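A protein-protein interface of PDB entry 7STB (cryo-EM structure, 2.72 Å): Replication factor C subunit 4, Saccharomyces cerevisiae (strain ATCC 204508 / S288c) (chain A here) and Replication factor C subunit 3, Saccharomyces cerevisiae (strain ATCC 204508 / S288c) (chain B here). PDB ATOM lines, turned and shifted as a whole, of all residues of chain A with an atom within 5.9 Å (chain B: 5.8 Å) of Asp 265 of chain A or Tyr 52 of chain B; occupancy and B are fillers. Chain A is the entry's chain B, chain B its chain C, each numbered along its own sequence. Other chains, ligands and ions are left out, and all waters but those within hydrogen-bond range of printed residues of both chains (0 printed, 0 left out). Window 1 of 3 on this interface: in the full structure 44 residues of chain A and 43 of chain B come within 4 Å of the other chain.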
ATOM      1  N   HIS A 232       3.046   2.293  -3.832  1.00  0.00           N
ATOM      2  CA  HIS A 232       4.376   2.875  -3.980  1.00  0.00           C
ATOM      3  C   HIS A 232       5.479   1.948  -3.482  1.00  0.00           C
ATOM      4  O   HIS A 232       6.508   1.827  -4.174  1.00  0.00           O
ATOM      5  CB  HIS A 232       4.404   4.225  -3.248  1.00  0.00           C
ATOM      6  CG  HIS A 232       5.491   5.147  -3.703  1.00  0.00           C
ATOM      7  ND1 HIS A 232       6.238   5.905  -2.829  1.00  0.00           N
ATOM      8  CD2 HIS A 232       5.945   5.447  -4.944  1.00  0.00           C
ATOM      9  CE1 HIS A 232       7.110   6.628  -3.509  1.00  0.00           C
ATOM     10  NE2 HIS A 232       6.953   6.367  -4.794  1.00  0.00           N
ATOM     11  N   GLY A 260       4.302  11.869 -10.667  1.00  0.00           N
ATOM     12  CA  GLY A 260       4.092  12.939  -9.712  1.00  0.00           C
ATOM     13  C   GLY A 260       4.423  12.557  -8.283  1.00  0.00           C
ATOM     14  O   GLY A 260       3.679  12.894  -7.358  1.00  0.00           O
ATOM     15  N   TYR A 261       5.536  11.856  -8.091  1.00  0.00           N
ATOM     16  CA  TYR A 261       6.007  11.474  -6.766  1.00  0.00           C
ATOM     17  C   TYR A 261       7.201  12.339  -6.388  1.00  0.00           C
ATOM     18  O   TYR A 261       8.152  12.468  -7.166  1.00  0.00           O
ATOM     19  CB  TYR A 261       6.388   9.995  -6.726  1.00  0.00           C
ATOM     20  CG  TYR A 261       5.203   9.059  -6.670  1.00  0.00           C
ATOM     21  CD1 TYR A 261       4.525   8.839  -5.480  1.00  0.00           C
ATOM     22  CD2 TYR A 261       4.763   8.395  -7.807  1.00  0.00           C
ATOM     23  CE1 TYR A 261       3.441   7.986  -5.423  1.00  0.00           C
ATOM     24  CE2 TYR A 261       3.681   7.540  -7.760  1.00  0.00           C
ATOM     25  CZ  TYR A 261       3.023   7.340  -6.565  1.00  0.00           C
ATOM     26  OH  TYR A 261       1.944   6.489  -6.512  1.00  0.00           O
ATOM     27  N   SER A 262       7.146  12.932  -5.198  1.00  0.00           N
ATOM     28  CA  SER A 262       8.230  13.789  -4.741  1.00  0.00           C
ATOM     29  C   SER A 262       9.472  12.964  -4.422  1.00  0.00           C
ATOM     30  O   SER A 262       9.392  11.786  -4.062  1.00  0.00           O
ATOM     31  CB  SER A 262       7.799  14.584  -3.508  1.00  0.00           C
ATOM     32  OG  SER A 262       7.239  13.739  -2.519  1.00  0.00           O
ATOM     33  N   SER A 263      10.636  13.603  -4.557  1.00  0.00           N
ATOM     34  CA  SER A 263      11.896  12.910  -4.310  1.00  0.00           C
ATOM     35  C   SER A 263      12.002  12.456  -2.859  1.00  0.00           C
ATOM     36  O   SER A 263      12.521  11.369  -2.577  1.00  0.00           O
ATOM     37  CB  SER A 263      13.070  13.819  -4.672  1.00  0.00           C
ATOM     38  OG  SER A 263      12.908  14.369  -5.967  1.00  0.00           O
ATOM     39  N   ILE A 264      11.531  13.281  -1.924  1.00  0.00           N
ATOM     40  CA  ILE A 264      11.629  12.932  -0.509  1.00  0.00           C
ATOM     41  C   ILE A 264      10.822  11.673  -0.215  1.00  0.00           C
ATOM     42  O   ILE A 264      11.276  10.782   0.517  1.00  0.00           O
ATOM     43  CB  ILE A 264      11.181  14.122   0.364  1.00  0.00           C
ATOM     44  CG1 ILE A 264      11.375  13.810   1.852  1.00  0.00           C
ATOM     45  CG2 ILE A 264       9.731  14.497   0.080  1.00  0.00           C
ATOM     46  CD1 ILE A 264      12.818  13.609   2.253  1.00  0.00           C
ATOM     47  N   ASP A 265       9.615  11.574  -0.778  1.00  0.00           N
ATOM     48  CA  ASP A 265       8.814  10.371  -0.589  1.00  0.00           C
ATOM     49  C   ASP A 265       9.526   9.148  -1.150  1.00  0.00           C
ATOM     50  O   ASP A 265       9.544   8.084  -0.517  1.00  0.00           O
ATOM     51  CB  ASP A 265       7.447  10.541  -1.251  1.00  0.00           C
ATOM     52  CG  ASP A 265       6.542  11.491  -0.489  1.00  0.00           C
ATOM     53  OD1 ASP A 265       6.608  11.506   0.757  1.00  0.00           O
ATOM     54  OD2 ASP A 265       5.764  12.220  -1.137  1.00  0.00           O
ATOM     55  N   ILE A 266      10.127   9.287  -2.333  1.00  0.00           N
ATOM     56  CA  ILE A 266      10.831   8.169  -2.953  1.00  0.00           C
ATOM     57  C   ILE A 266      11.986   7.713  -2.073  1.00  0.00           C
ATOM     58  O   ILE A 266      12.193   6.512  -1.869  1.00  0.00           O
ATOM     59  CB  ILE A 266      11.310   8.554  -4.365  1.00  0.00           C
ATOM     60  CG1 ILE A 266      10.106   8.781  -5.285  1.00  0.00           C
ATOM     61  CG2 ILE A 266      12.219   7.474  -4.934  1.00  0.00           C
ATOM     62  CD1 ILE A 266      10.430   9.548  -6.547  1.00  0.00           C
ATOM     63  N   VAL A 267      12.757   8.660  -1.534  1.00  0.00           N
ATOM     64  CA  VAL A 267      13.898   8.294  -0.698  1.00  0.00           C
ATOM     65  C   VAL A 267      13.434   7.621   0.590  1.00  0.00           C
ATOM     66  O   VAL A 267      14.015   6.617   1.026  1.00  0.00           O
ATOM     67  CB  VAL A 267      14.768   9.531  -0.413  1.00  0.00           C
ATOM     68  CG1 VAL A 267      15.707   9.263   0.750  1.00  0.00           C
ATOM     69  CG2 VAL A 267      15.554   9.920  -1.653  1.00  0.00           C
ATOM     70  N   THR A 268      12.393   8.160   1.231  1.00  0.00           N
ATOM     71  CA  THR A 268      11.913   7.551   2.470  1.00  0.00           C
ATOM     72  C   THR A 268      11.404   6.135   2.230  1.00  0.00           C
ATOM     73  O   THR A 268      11.713   5.216   3.002  1.00  0.00           O
ATOM     74  CB  THR A 268      10.820   8.414   3.103  1.00  0.00           C
ATOM     75  OG1 THR A 268       9.707   8.520   2.202  1.00  0.00           O
ATOM     76  CG2 THR A 268      11.353   9.798   3.466  1.00  0.00           C
ATOM     77  N   THR A 269      10.629   5.932   1.163  1.00  0.00           N
ATOM     78  CA  THR A 269      10.131   4.590   0.878  1.00  0.00           C
ATOM     79  C   THR A 269      11.269   3.653   0.482  1.00  0.00           C
ATOM     80  O   THR A 269      11.232   2.460   0.795  1.00  0.00           O
ATOM     81  CB  THR A 269       9.055   4.638  -0.209  1.00  0.00           C
ATOM     82  OG1 THR A 269       8.509   3.328  -0.406  1.00  0.00           O
ATOM     83  CG2 THR A 269       9.618   5.144  -1.508  1.00  0.00           C
ATOM     84  N   SER A 270      12.289   4.172  -0.209  1.00  0.00           N
ATOM     85  CA  SER A 270      13.452   3.352  -0.530  1.00  0.00           C
ATOM     86  C   SER A 270      14.148   2.875   0.737  1.00  0.00           C
ATOM     87  O   SER A 270      14.518   1.701   0.849  1.00  0.00           O
ATOM     88  CB  SER A 270      14.424   4.144  -1.404  1.00  0.00           C
ATOM     89  OG  SER A 270      13.851   4.441  -2.664  1.00  0.00           O
ATOM     90  N   LEU B  50      -8.262  12.921  -0.873  1.00  0.00           N
ATOM     91  CA  LEU B  50      -6.863  13.253  -0.617  1.00  0.00           C
ATOM     92  C   LEU B  50      -6.204  13.507  -1.968  1.00  0.00           C
ATOM     93  O   LEU B  50      -5.820  12.564  -2.663  1.00  0.00           O
ATOM     94  CB  LEU B  50      -6.158  12.138   0.150  1.00  0.00           C
ATOM     95  CG  LEU B  50      -4.736  12.439   0.637  1.00  0.00           C
ATOM     96  CD1 LEU B  50      -4.417  11.608   1.867  1.00  0.00           C
ATOM     97  CD2 LEU B  50      -3.703  12.185  -0.453  1.00  0.00           C
ATOM     98  N   PHE B  51      -6.080  14.779  -2.335  1.00  0.00           N
ATOM     99  CA  PHE B  51      -5.436  15.176  -3.581  1.00  0.00           C
ATOM    100  C   PHE B  51      -3.935  15.274  -3.335  1.00  0.00           C
ATOM    101  O   PHE B  51      -3.466  16.202  -2.665  1.00  0.00           O
ATOM    102  CB  PHE B  51      -5.996  16.505  -4.084  1.00  0.00           C
ATOM    103  CG  PHE B  51      -7.437  16.444  -4.525  1.00  0.00           C
ATOM    104  CD1 PHE B  51      -8.144  15.249  -4.513  1.00  0.00           C
ATOM    105  CD2 PHE B  51      -8.084  17.589  -4.959  1.00  0.00           C
ATOM    106  CE1 PHE B  51      -9.463  15.204  -4.920  1.00  0.00           C
ATOM    107  CE2 PHE B  51      -9.402  17.548  -5.368  1.00  0.00           C
ATOM    108  CZ  PHE B  51     -10.092  16.355  -5.348  1.00  0.00           C
ATOM    109  N   TYR B  52      -3.183  14.321  -3.877  1.00  0.00           N
ATOM    110  CA  TYR B  52      -1.737  14.275  -3.718  1.00  0.00           C
ATOM    111  C   TYR B  52      -1.083  14.582  -5.056  1.00  0.00           C
ATOM    112  O   TYR B  52      -1.406  13.949  -6.066  1.00  0.00           O
ATOM    113  CB  TYR B  52      -1.286  12.905  -3.207  1.00  0.00           C
ATOM    114  CG  TYR B  52       0.201  12.668  -3.323  1.00  0.00           C
ATOM    115  CD1 TYR B  52       1.080  13.184  -2.382  1.00  0.00           C
ATOM    116  CD2 TYR B  52       0.726  11.929  -4.374  1.00  0.00           C
ATOM    117  CE1 TYR B  52       2.440  12.971  -2.484  1.00  0.00           C
ATOM    118  CE2 TYR B  52       2.084  11.711  -4.485  1.00  0.00           C
ATOM    119  CZ  TYR B  52       2.938  12.235  -3.537  1.00  0.00           C
ATOM    120  OH  TYR B  52       4.292  12.020  -3.642  1.00  0.00           O
ATOM    121  N   GLY B  53      -0.174  15.552  -5.067  1.00  0.00           N
ATOM    122  CA  GLY B  53       0.502  15.911  -6.292  1.00  0.00           C
ATOM    123  C   GLY B  53       1.522  17.020  -6.135  1.00  0.00           C
ATOM    124  O   GLY B  53       1.605  17.684  -5.097  1.00  0.00           O
ATOM    125  N   PRO B  54       2.315  17.245  -7.178  1.00  0.00           N
ATOM    126  CA  PRO B  54       3.349  18.282  -7.120  1.00  0.00           C
ATOM    127  C   PRO B  54       2.745  19.670  -7.238  1.00  0.00           C
ATOM    128  O   PRO B  54       1.535  19.817  -7.467  1.00  0.00           O
ATOM    129  CB  PRO B  54       4.244  17.955  -8.325  1.00  0.00           C
ATOM    130  CG  PRO B  54       3.361  17.232  -9.268  1.00  0.00           C
ATOM    131  CD  PRO B  54       2.357  16.486  -8.440  1.00  0.00           C
ATOM    132  N   LYS B  59      -4.906  21.326  -7.762  1.00  0.00           N
ATOM    133  CA  LYS B  59      -5.621  20.736  -6.636  1.00  0.00           C
ATOM    134  C   LYS B  59      -6.497  21.770  -5.938  1.00  0.00           C
ATOM    135  O   LYS B  59      -7.699  21.552  -5.750  1.00  0.00           O
ATOM    136  CB  LYS B  59      -4.625  20.126  -5.649  1.00  0.00           C
ATOM    137  CG  LYS B  59      -3.635  19.163  -6.282  1.00  0.00           C
ATOM    138  CD  LYS B  59      -2.824  18.420  -5.230  1.00  0.00           C
ATOM    139  CE  LYS B  59      -1.753  19.308  -4.615  1.00  0.00           C
ATOM    140  NZ  LYS B  59      -0.678  19.651  -5.587  1.00  0.00           N
ATOM    141  N   VAL B 145      -8.066  16.747   1.708  1.00  0.00           N
ATOM    142  CA  VAL B 145      -6.700  16.959   2.169  1.00  0.00           C
ATOM    143  C   VAL B 145      -5.808  17.091   0.944  1.00  0.00           C
ATOM    144  O   VAL B 145      -5.700  16.154   0.147  1.00  0.00           O
ATOM    145  CB  VAL B 145      -6.224  15.810   3.073  1.00  0.00           C
ATOM    146  CG1 VAL B 145      -4.713  15.833   3.215  1.00  0.00           C
ATOM    147  CG2 VAL B 145      -6.895  15.893   4.434  1.00  0.00           C
ATOM    148  N   LEU B 146      -5.159  18.242   0.802  1.00  0.00           N
ATOM    149  CA  LEU B 146      -4.261  18.503  -0.315  1.00  0.00           C
ATOM    150  C   LEU B 146      -2.823  18.384   0.165  1.00  0.00           C
ATOM    151  O   LEU B 146      -2.467  18.939   1.210  1.00  0.00           O
ATOM    152  CB  LEU B 146      -4.514  19.892  -0.903  1.00  0.00           C
ATOM    153  CG  LEU B 146      -5.781  20.036  -1.748  1.00  0.00           C
ATOM    154  CD1 LEU B 146      -7.023  20.062  -0.872  1.00  0.00           C
ATOM    155  CD2 LEU B 146      -5.702  21.289  -2.602  1.00  0.00           C
ATOM    156  N   ALA B 147      -2.000  17.657  -0.590  1.00  0.00           N
ATOM    157  CA  ALA B 147      -0.632  17.415  -0.159  1.00  0.00           C
ATOM    158  C   ALA B 147       0.296  17.282  -1.358  1.00  0.00           C
ATOM    159  O   ALA B 147      -0.122  16.903  -2.458  1.00  0.00           O
ATOM    160  CB  ALA B 147      -0.539  16.155   0.710  1.00  0.00           C
ATOM    161  N   ASN B 148       1.568  17.611  -1.122  1.00  0.00           N
ATOM    162  CA  ASN B 148       2.645  17.350  -2.065  1.00  0.00           C
ATOM    163  C   ASN B 148       3.620  16.291  -1.576  1.00  0.00           C
ATOM    164  O   ASN B 148       4.377  15.752  -2.388  1.00  0.00           O
ATOM    165  CB  ASN B 148       3.429  18.638  -2.357  1.00  0.00           C
ATOM    166  CG  ASN B 148       2.532  19.798  -2.739  1.00  0.00           C
ATOM    167  OD1 ASN B 148       1.816  20.346  -1.902  1.00  0.00           O
ATOM    168  ND2 ASN B 148       2.572  20.182  -4.008  1.00  0.00           N
ATOM    169  N   TYR B 149       3.617  15.983  -0.278  1.00  0.00           N
ATOM    170  CA  TYR B 149       4.510  14.990   0.310  1.00  0.00           C
ATOM    171  C   TYR B 149       3.673  14.075   1.194  1.00  0.00           C
ATOM    172  O   TYR B 149       3.173  14.504   2.239  1.00  0.00           O
ATOM    173  CB  TYR B 149       5.623  15.658   1.117  1.00  0.00           C
ATOM    174  CG  TYR B 149       6.191  16.896   0.464  1.00  0.00           C
ATOM    175  CD1 TYR B 149       6.928  16.812  -0.708  1.00  0.00           C
ATOM    176  CD2 TYR B 149       5.987  18.152   1.021  1.00  0.00           C
ATOM    177  CE1 TYR B 149       7.447  17.942  -1.308  1.00  0.00           C
ATOM    178  CE2 TYR B 149       6.502  19.288   0.428  1.00  0.00           C
ATOM    179  CZ  TYR B 149       7.230  19.177  -0.735  1.00  0.00           C
ATOM    180  OH  TYR B 149       7.745  20.307  -1.328  1.00  0.00           O
ATOM    181  N   ALA B 150       3.523  12.817   0.779  1.00  0.00           N
ATOM    182  CA  ALA B 150       2.674  11.887   1.515  1.00  0.00           C
ATOM    183  C   ALA B 150       3.336  11.383   2.792  1.00  0.00           C
ATOM    184  O   ALA B 150       2.639  11.099   3.771  1.00  0.00           O
ATOM    185  CB  ALA B 150       2.300  10.703   0.624  1.00  0.00           C
ATOM    186  N   HIS B 151       4.665  11.269   2.807  1.00  0.00           N
ATOM    187  CA  HIS B 151       5.349  10.701   3.963  1.00  0.00           C
ATOM    188  C   HIS B 151       5.160  11.540   5.221  1.00  0.00           C
ATOM    189  O   HIS B 151       5.350  11.022   6.327  1.00  0.00           O
ATOM    190  CB  HIS B 151       6.838  10.540   3.662  1.00  0.00           C
ATOM    191  CG  HIS B 151       7.599  11.828   3.671  1.00  0.00           C
ATOM    192  ND1 HIS B 151       7.508  12.751   2.652  1.00  0.00           N
ATOM    193  CD2 HIS B 151       8.468  12.343   4.571  1.00  0.00           C
ATOM    194  CE1 HIS B 151       8.285  13.784   2.928  1.00  0.00           C
ATOM    195  NE2 HIS B 151       8.881  13.559   4.085  1.00  0.00           N
ATOM    196  N   LYS B 152       4.797  12.814   5.084  1.00  0.00           N
ATOM    197  CA  LYS B 152       4.454  13.642   6.234  1.00  0.00           C
ATOM    198  C   LYS B 152       3.064  13.350   6.781  1.00  0.00           C
ATOM    199  O   LYS B 152       2.711  13.882   7.838  1.00  0.00           O
ATOM    200  CB  LYS B 152       4.551  15.128   5.870  1.00  0.00           C
ATOM    201  CG  LYS B 152       5.933  15.608   5.455  1.00  0.00           C
ATOM    202  CD  LYS B 152       6.892  15.596   6.638  1.00  0.00           C
ATOM    203  CE  LYS B 152       8.283  16.069   6.250  1.00  0.00           C
ATOM    204  NZ  LYS B 152       8.305  17.515   5.901  1.00  0.00           N
ATOM    205  N   ARG B 163      -7.602   8.350  -2.150  1.00  0.00           N
ATOM    206  CA  ARG B 163      -6.466   9.062  -2.722  1.00  0.00           C
ATOM    207  C   ARG B 163      -6.681   9.316  -4.207  1.00  0.00           C
ATOM    208  O   ARG B 163      -7.051   8.405  -4.954  1.00  0.00           O
ATOM    209  CB  ARG B 163      -5.179   8.264  -2.505  1.00  0.00           C
ATOM    210  CG  ARG B 163      -3.964   8.830  -3.222  1.00  0.00           C
ATOM    211  CD  ARG B 163      -2.689   8.138  -2.775  1.00  0.00           C
ATOM    212  NE  ARG B 163      -1.523   8.596  -3.522  1.00  0.00           N
ATOM    213  CZ  ARG B 163      -1.067   8.033  -4.634  1.00  0.00           C
ATOM    214  NH1 ARG B 163      -1.665   6.983  -5.174  1.00  0.00           N
ATOM    215  NH2 ARG B 163       0.016   8.536  -5.219  1.00  0.00           N
ATOM    216  N   PHE B 164      -6.450  10.558  -4.627  1.00  0.00           N
ATOM    217  CA  PHE B 164      -6.444  10.947  -6.031  1.00  0.00           C
ATOM    218  C   PHE B 164      -5.098  11.587  -6.335  1.00  0.00           C
ATOM    219  O   PHE B 164      -4.703  12.555  -5.674  1.00  0.00           O
ATOM    220  CB  PHE B 164      -7.585  11.917  -6.343  1.00  0.00           C
ATOM    221  CG  PHE B 164      -8.926  11.254  -6.477  1.00  0.00           C
ATOM    222  CD1 PHE B 164      -9.306  10.666  -7.670  1.00  0.00           C
ATOM    223  CD2 PHE B 164      -9.808  11.225  -5.410  1.00  0.00           C
ATOM    224  CE1 PHE B 164     -10.538  10.058  -7.797  1.00  0.00           C
ATOM    225  CE2 PHE B 164     -11.041  10.617  -5.532  1.00  0.00           C
ATOM    226  CZ  PHE B 164     -11.407  10.033  -6.728  1.00  0.00           C
ATOM    227  N   ARG B 165      -4.406  11.055  -7.337  1.00  0.00           N
ATOM    228  CA  ARG B 165      -3.076  11.519  -7.706  1.00  0.00           C
ATOM    229  C   ARG B 165      -3.196  12.508  -8.857  1.00  0.00           C
ATOM    230  O   ARG B 165      -3.753  12.178  -9.910  1.00  0.00           O
ATOM    231  CB  ARG B 165      -2.183  10.342  -8.100  1.00  0.00           C
ATOM    232  CG  ARG B 165      -0.699  10.668  -8.101  1.00  0.00           C
ATOM    233  CD  ARG B 165       0.112   9.595  -8.810  1.00  0.00           C
ATOM    234  NE  ARG B 165       0.032   9.711 -10.262  1.00  0.00           N
ATOM    235  CZ  ARG B 165      -0.810   9.035 -11.033  1.00  0.00           C
ATOM    236  NH1 ARG B 165      -1.684   8.180 -10.525  1.00  0.00           N
ATOM    237  NH2 ARG B 165      -0.776   9.220 -12.349  1.00  0.00           N
ATOM    238  N   PHE B 166      -2.676  13.715  -8.652  1.00  0.00           N
ATOM    239  CA  PHE B 166      -2.675  14.754  -9.679  1.00  0.00           C
ATOM    240  C   PHE B 166      -1.358  14.655 -10.440  1.00  0.00           C
ATOM    241  O   PHE B 166      -0.326  15.156  -9.989  1.00  0.00           O
ATOM    242  CB  PHE B 166      -2.857  16.131  -9.053  1.00  0.00           C
ATOM    243  CG  PHE B 166      -4.294  16.518  -8.848  1.00  0.00           C
ATOM    244  CD1 PHE B 166      -5.074  15.862  -7.912  1.00  0.00           C
ATOM    245  CD2 PHE B 166      -4.863  17.537  -9.591  1.00  0.00           C
ATOM    246  CE1 PHE B 166      -6.394  16.217  -7.721  1.00  0.00           C
ATOM    247  CE2 PHE B 166      -6.182  17.895  -9.406  1.00  0.00           C
ATOM    248  CZ  PHE B 166      -6.949  17.235  -8.470  1.00  0.00           C
ATOM    249  N   GLN B 167      -1.396  14.008 -11.599  1.00  0.00           N
ATOM    250  CA  GLN B 167      -0.202  13.842 -12.404  1.00  0.00           C
ATOM    251  C   GLN B 167       0.240  15.185 -12.979  1.00  0.00           C
ATOM    252  O   GLN B 167      -0.551  16.128 -13.057  1.00  0.00           O
ATOM    253  CB  GLN B 167      -0.460  12.853 -13.538  1.00  0.00           C
ATOM    254  CG  GLN B 167      -1.471  13.349 -14.562  1.00  0.00           C
ATOM    255  CD  GLN B 167      -1.969  12.246 -15.473  1.00  0.00           C
ATOM    256  OE1 GLN B 167      -2.875  11.494 -15.118  1.00  0.00           O
ATOM    257  NE2 GLN B 167      -1.380  12.148 -16.660  1.00  0.00           N
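The side-chain carboxylate (OD2) of Asp 265 of chain A is in hydrogen-bond range of the side-chain hydroxyl (OH) of Tyr 52 of chain B (2.9 Å). The backbone NH (N) of Ser 262 of chain A is in hydrogen-bond range of the side-chain hydroxyl (OH) of Tyr 52 of chain B (3.4 Å). OD2 of Asp 265 of chain A sits at hydrogen-bond distance from N of Ala 150 of chain B (3.0 Å). OH of Tyr 261 of chain A is in hydrogen-bond range of NH2 of Arg 163 of chain B (3.1 Å). OD1 of Asp 265 of chain A lies within hydrogen-bond range of ND1 of His 151 of chain B (2.4 Å).
The backbone carbonyl oxygen of Pro 54 of chain B is in hydrogen-bond range of the side-chain amino group of Lys 59 of chain B (2.9 Å). The side-chain hydroxyl (OG1) of Thr 268 of chain A lies close to the backbone carbonyl oxygen (O) of Ile 264 of chain A. The backbone NH (N) of Phe 166 of chain B sits at hydrogen-bond distance from the backbone carbonyl oxygen (O) of Tyr 52 of chain B, at 2.9 Å. O of Gly 53 of chain B is in hydrogen-bond range of ND2 of Asn 148 of chain B, at 2.9 Å. The side-chain hydroxyl (OG) of Ser 262 of chain A lies within hydrogen-bond range of the side-chain carboxylate (OD2) of Asp 265 of chain A (2.5 Å). The backbone NH (N) of Tyr 52 of chain B lies within hydrogen-bond range of the backbone carbonyl oxygen (O) of Phe 164 of chain B (2.9 Å).
Among the printed residues, merely in contact across the chains: Ile 264 of chain A with His 151 of chain B (3.3 Å), Asp 265 of chain A with Tyr 149 of chain B (3.4 Å), Gly 260 of chain A with Tyr 52 of chain B (3.5 Å), Ser 262 of chain A with Asn 148 of chain B (3.5 Å), Ser 262 of chain A with Tyr 149 of chain B (3.6 Å), Tyr 261 of chain A with Tyr 52 of chain B (3.6 Å), Ile 264 of chain A with Tyr 149 of chain B (3.7 Å), Thr 268 of chain A with His 151 of chain B (3.8 Å), Gly 260 of chain A with Pro 54 of chain B (3.98 Å) and Asp 265 of chain A with Asn 148 of chain B (3.995 Å).
Of the printed residues of chain B, Asp 265 of chain A touches Tyr 52 (2.9 Å), Asn 148 (3.995 Å), Tyr 149 (3.4 Å), Ala 150 (3.0 Å) and His 151 (2.4 Å). Of the printed residues of chain B, Ser 262 of chain A touches Tyr 52 (3.4 Å), Asn 148 (3.5 Å) and Tyr 149 (3.6 Å). Of the printed residues of chain A, Tyr 149 of chain B touches Ser 262 (3.6 Å), Ile 264 (3.7 Å) and Asp 265 (3.4 Å). Gln 167 of chain B touches none of the printed residues of chain A.
Printed residues of chain B that touch a printed residue of chain A: Tyr 52, Pro 54, Asn 148, Tyr 149, Ala 150, His 151 and Arg 163. Printed residues of chain A that touch a printed residue of chain B: Gly 260, Tyr 261, Ser 262, Ile 264, Asp 265 and Thr 268. Among the printed residues, 15 pairs touch across the chains. Among the printed residues, no Asp or Glu carboxylate lies within 4 Å of a Lys or Arg side-chain nitrogen of the other chain.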
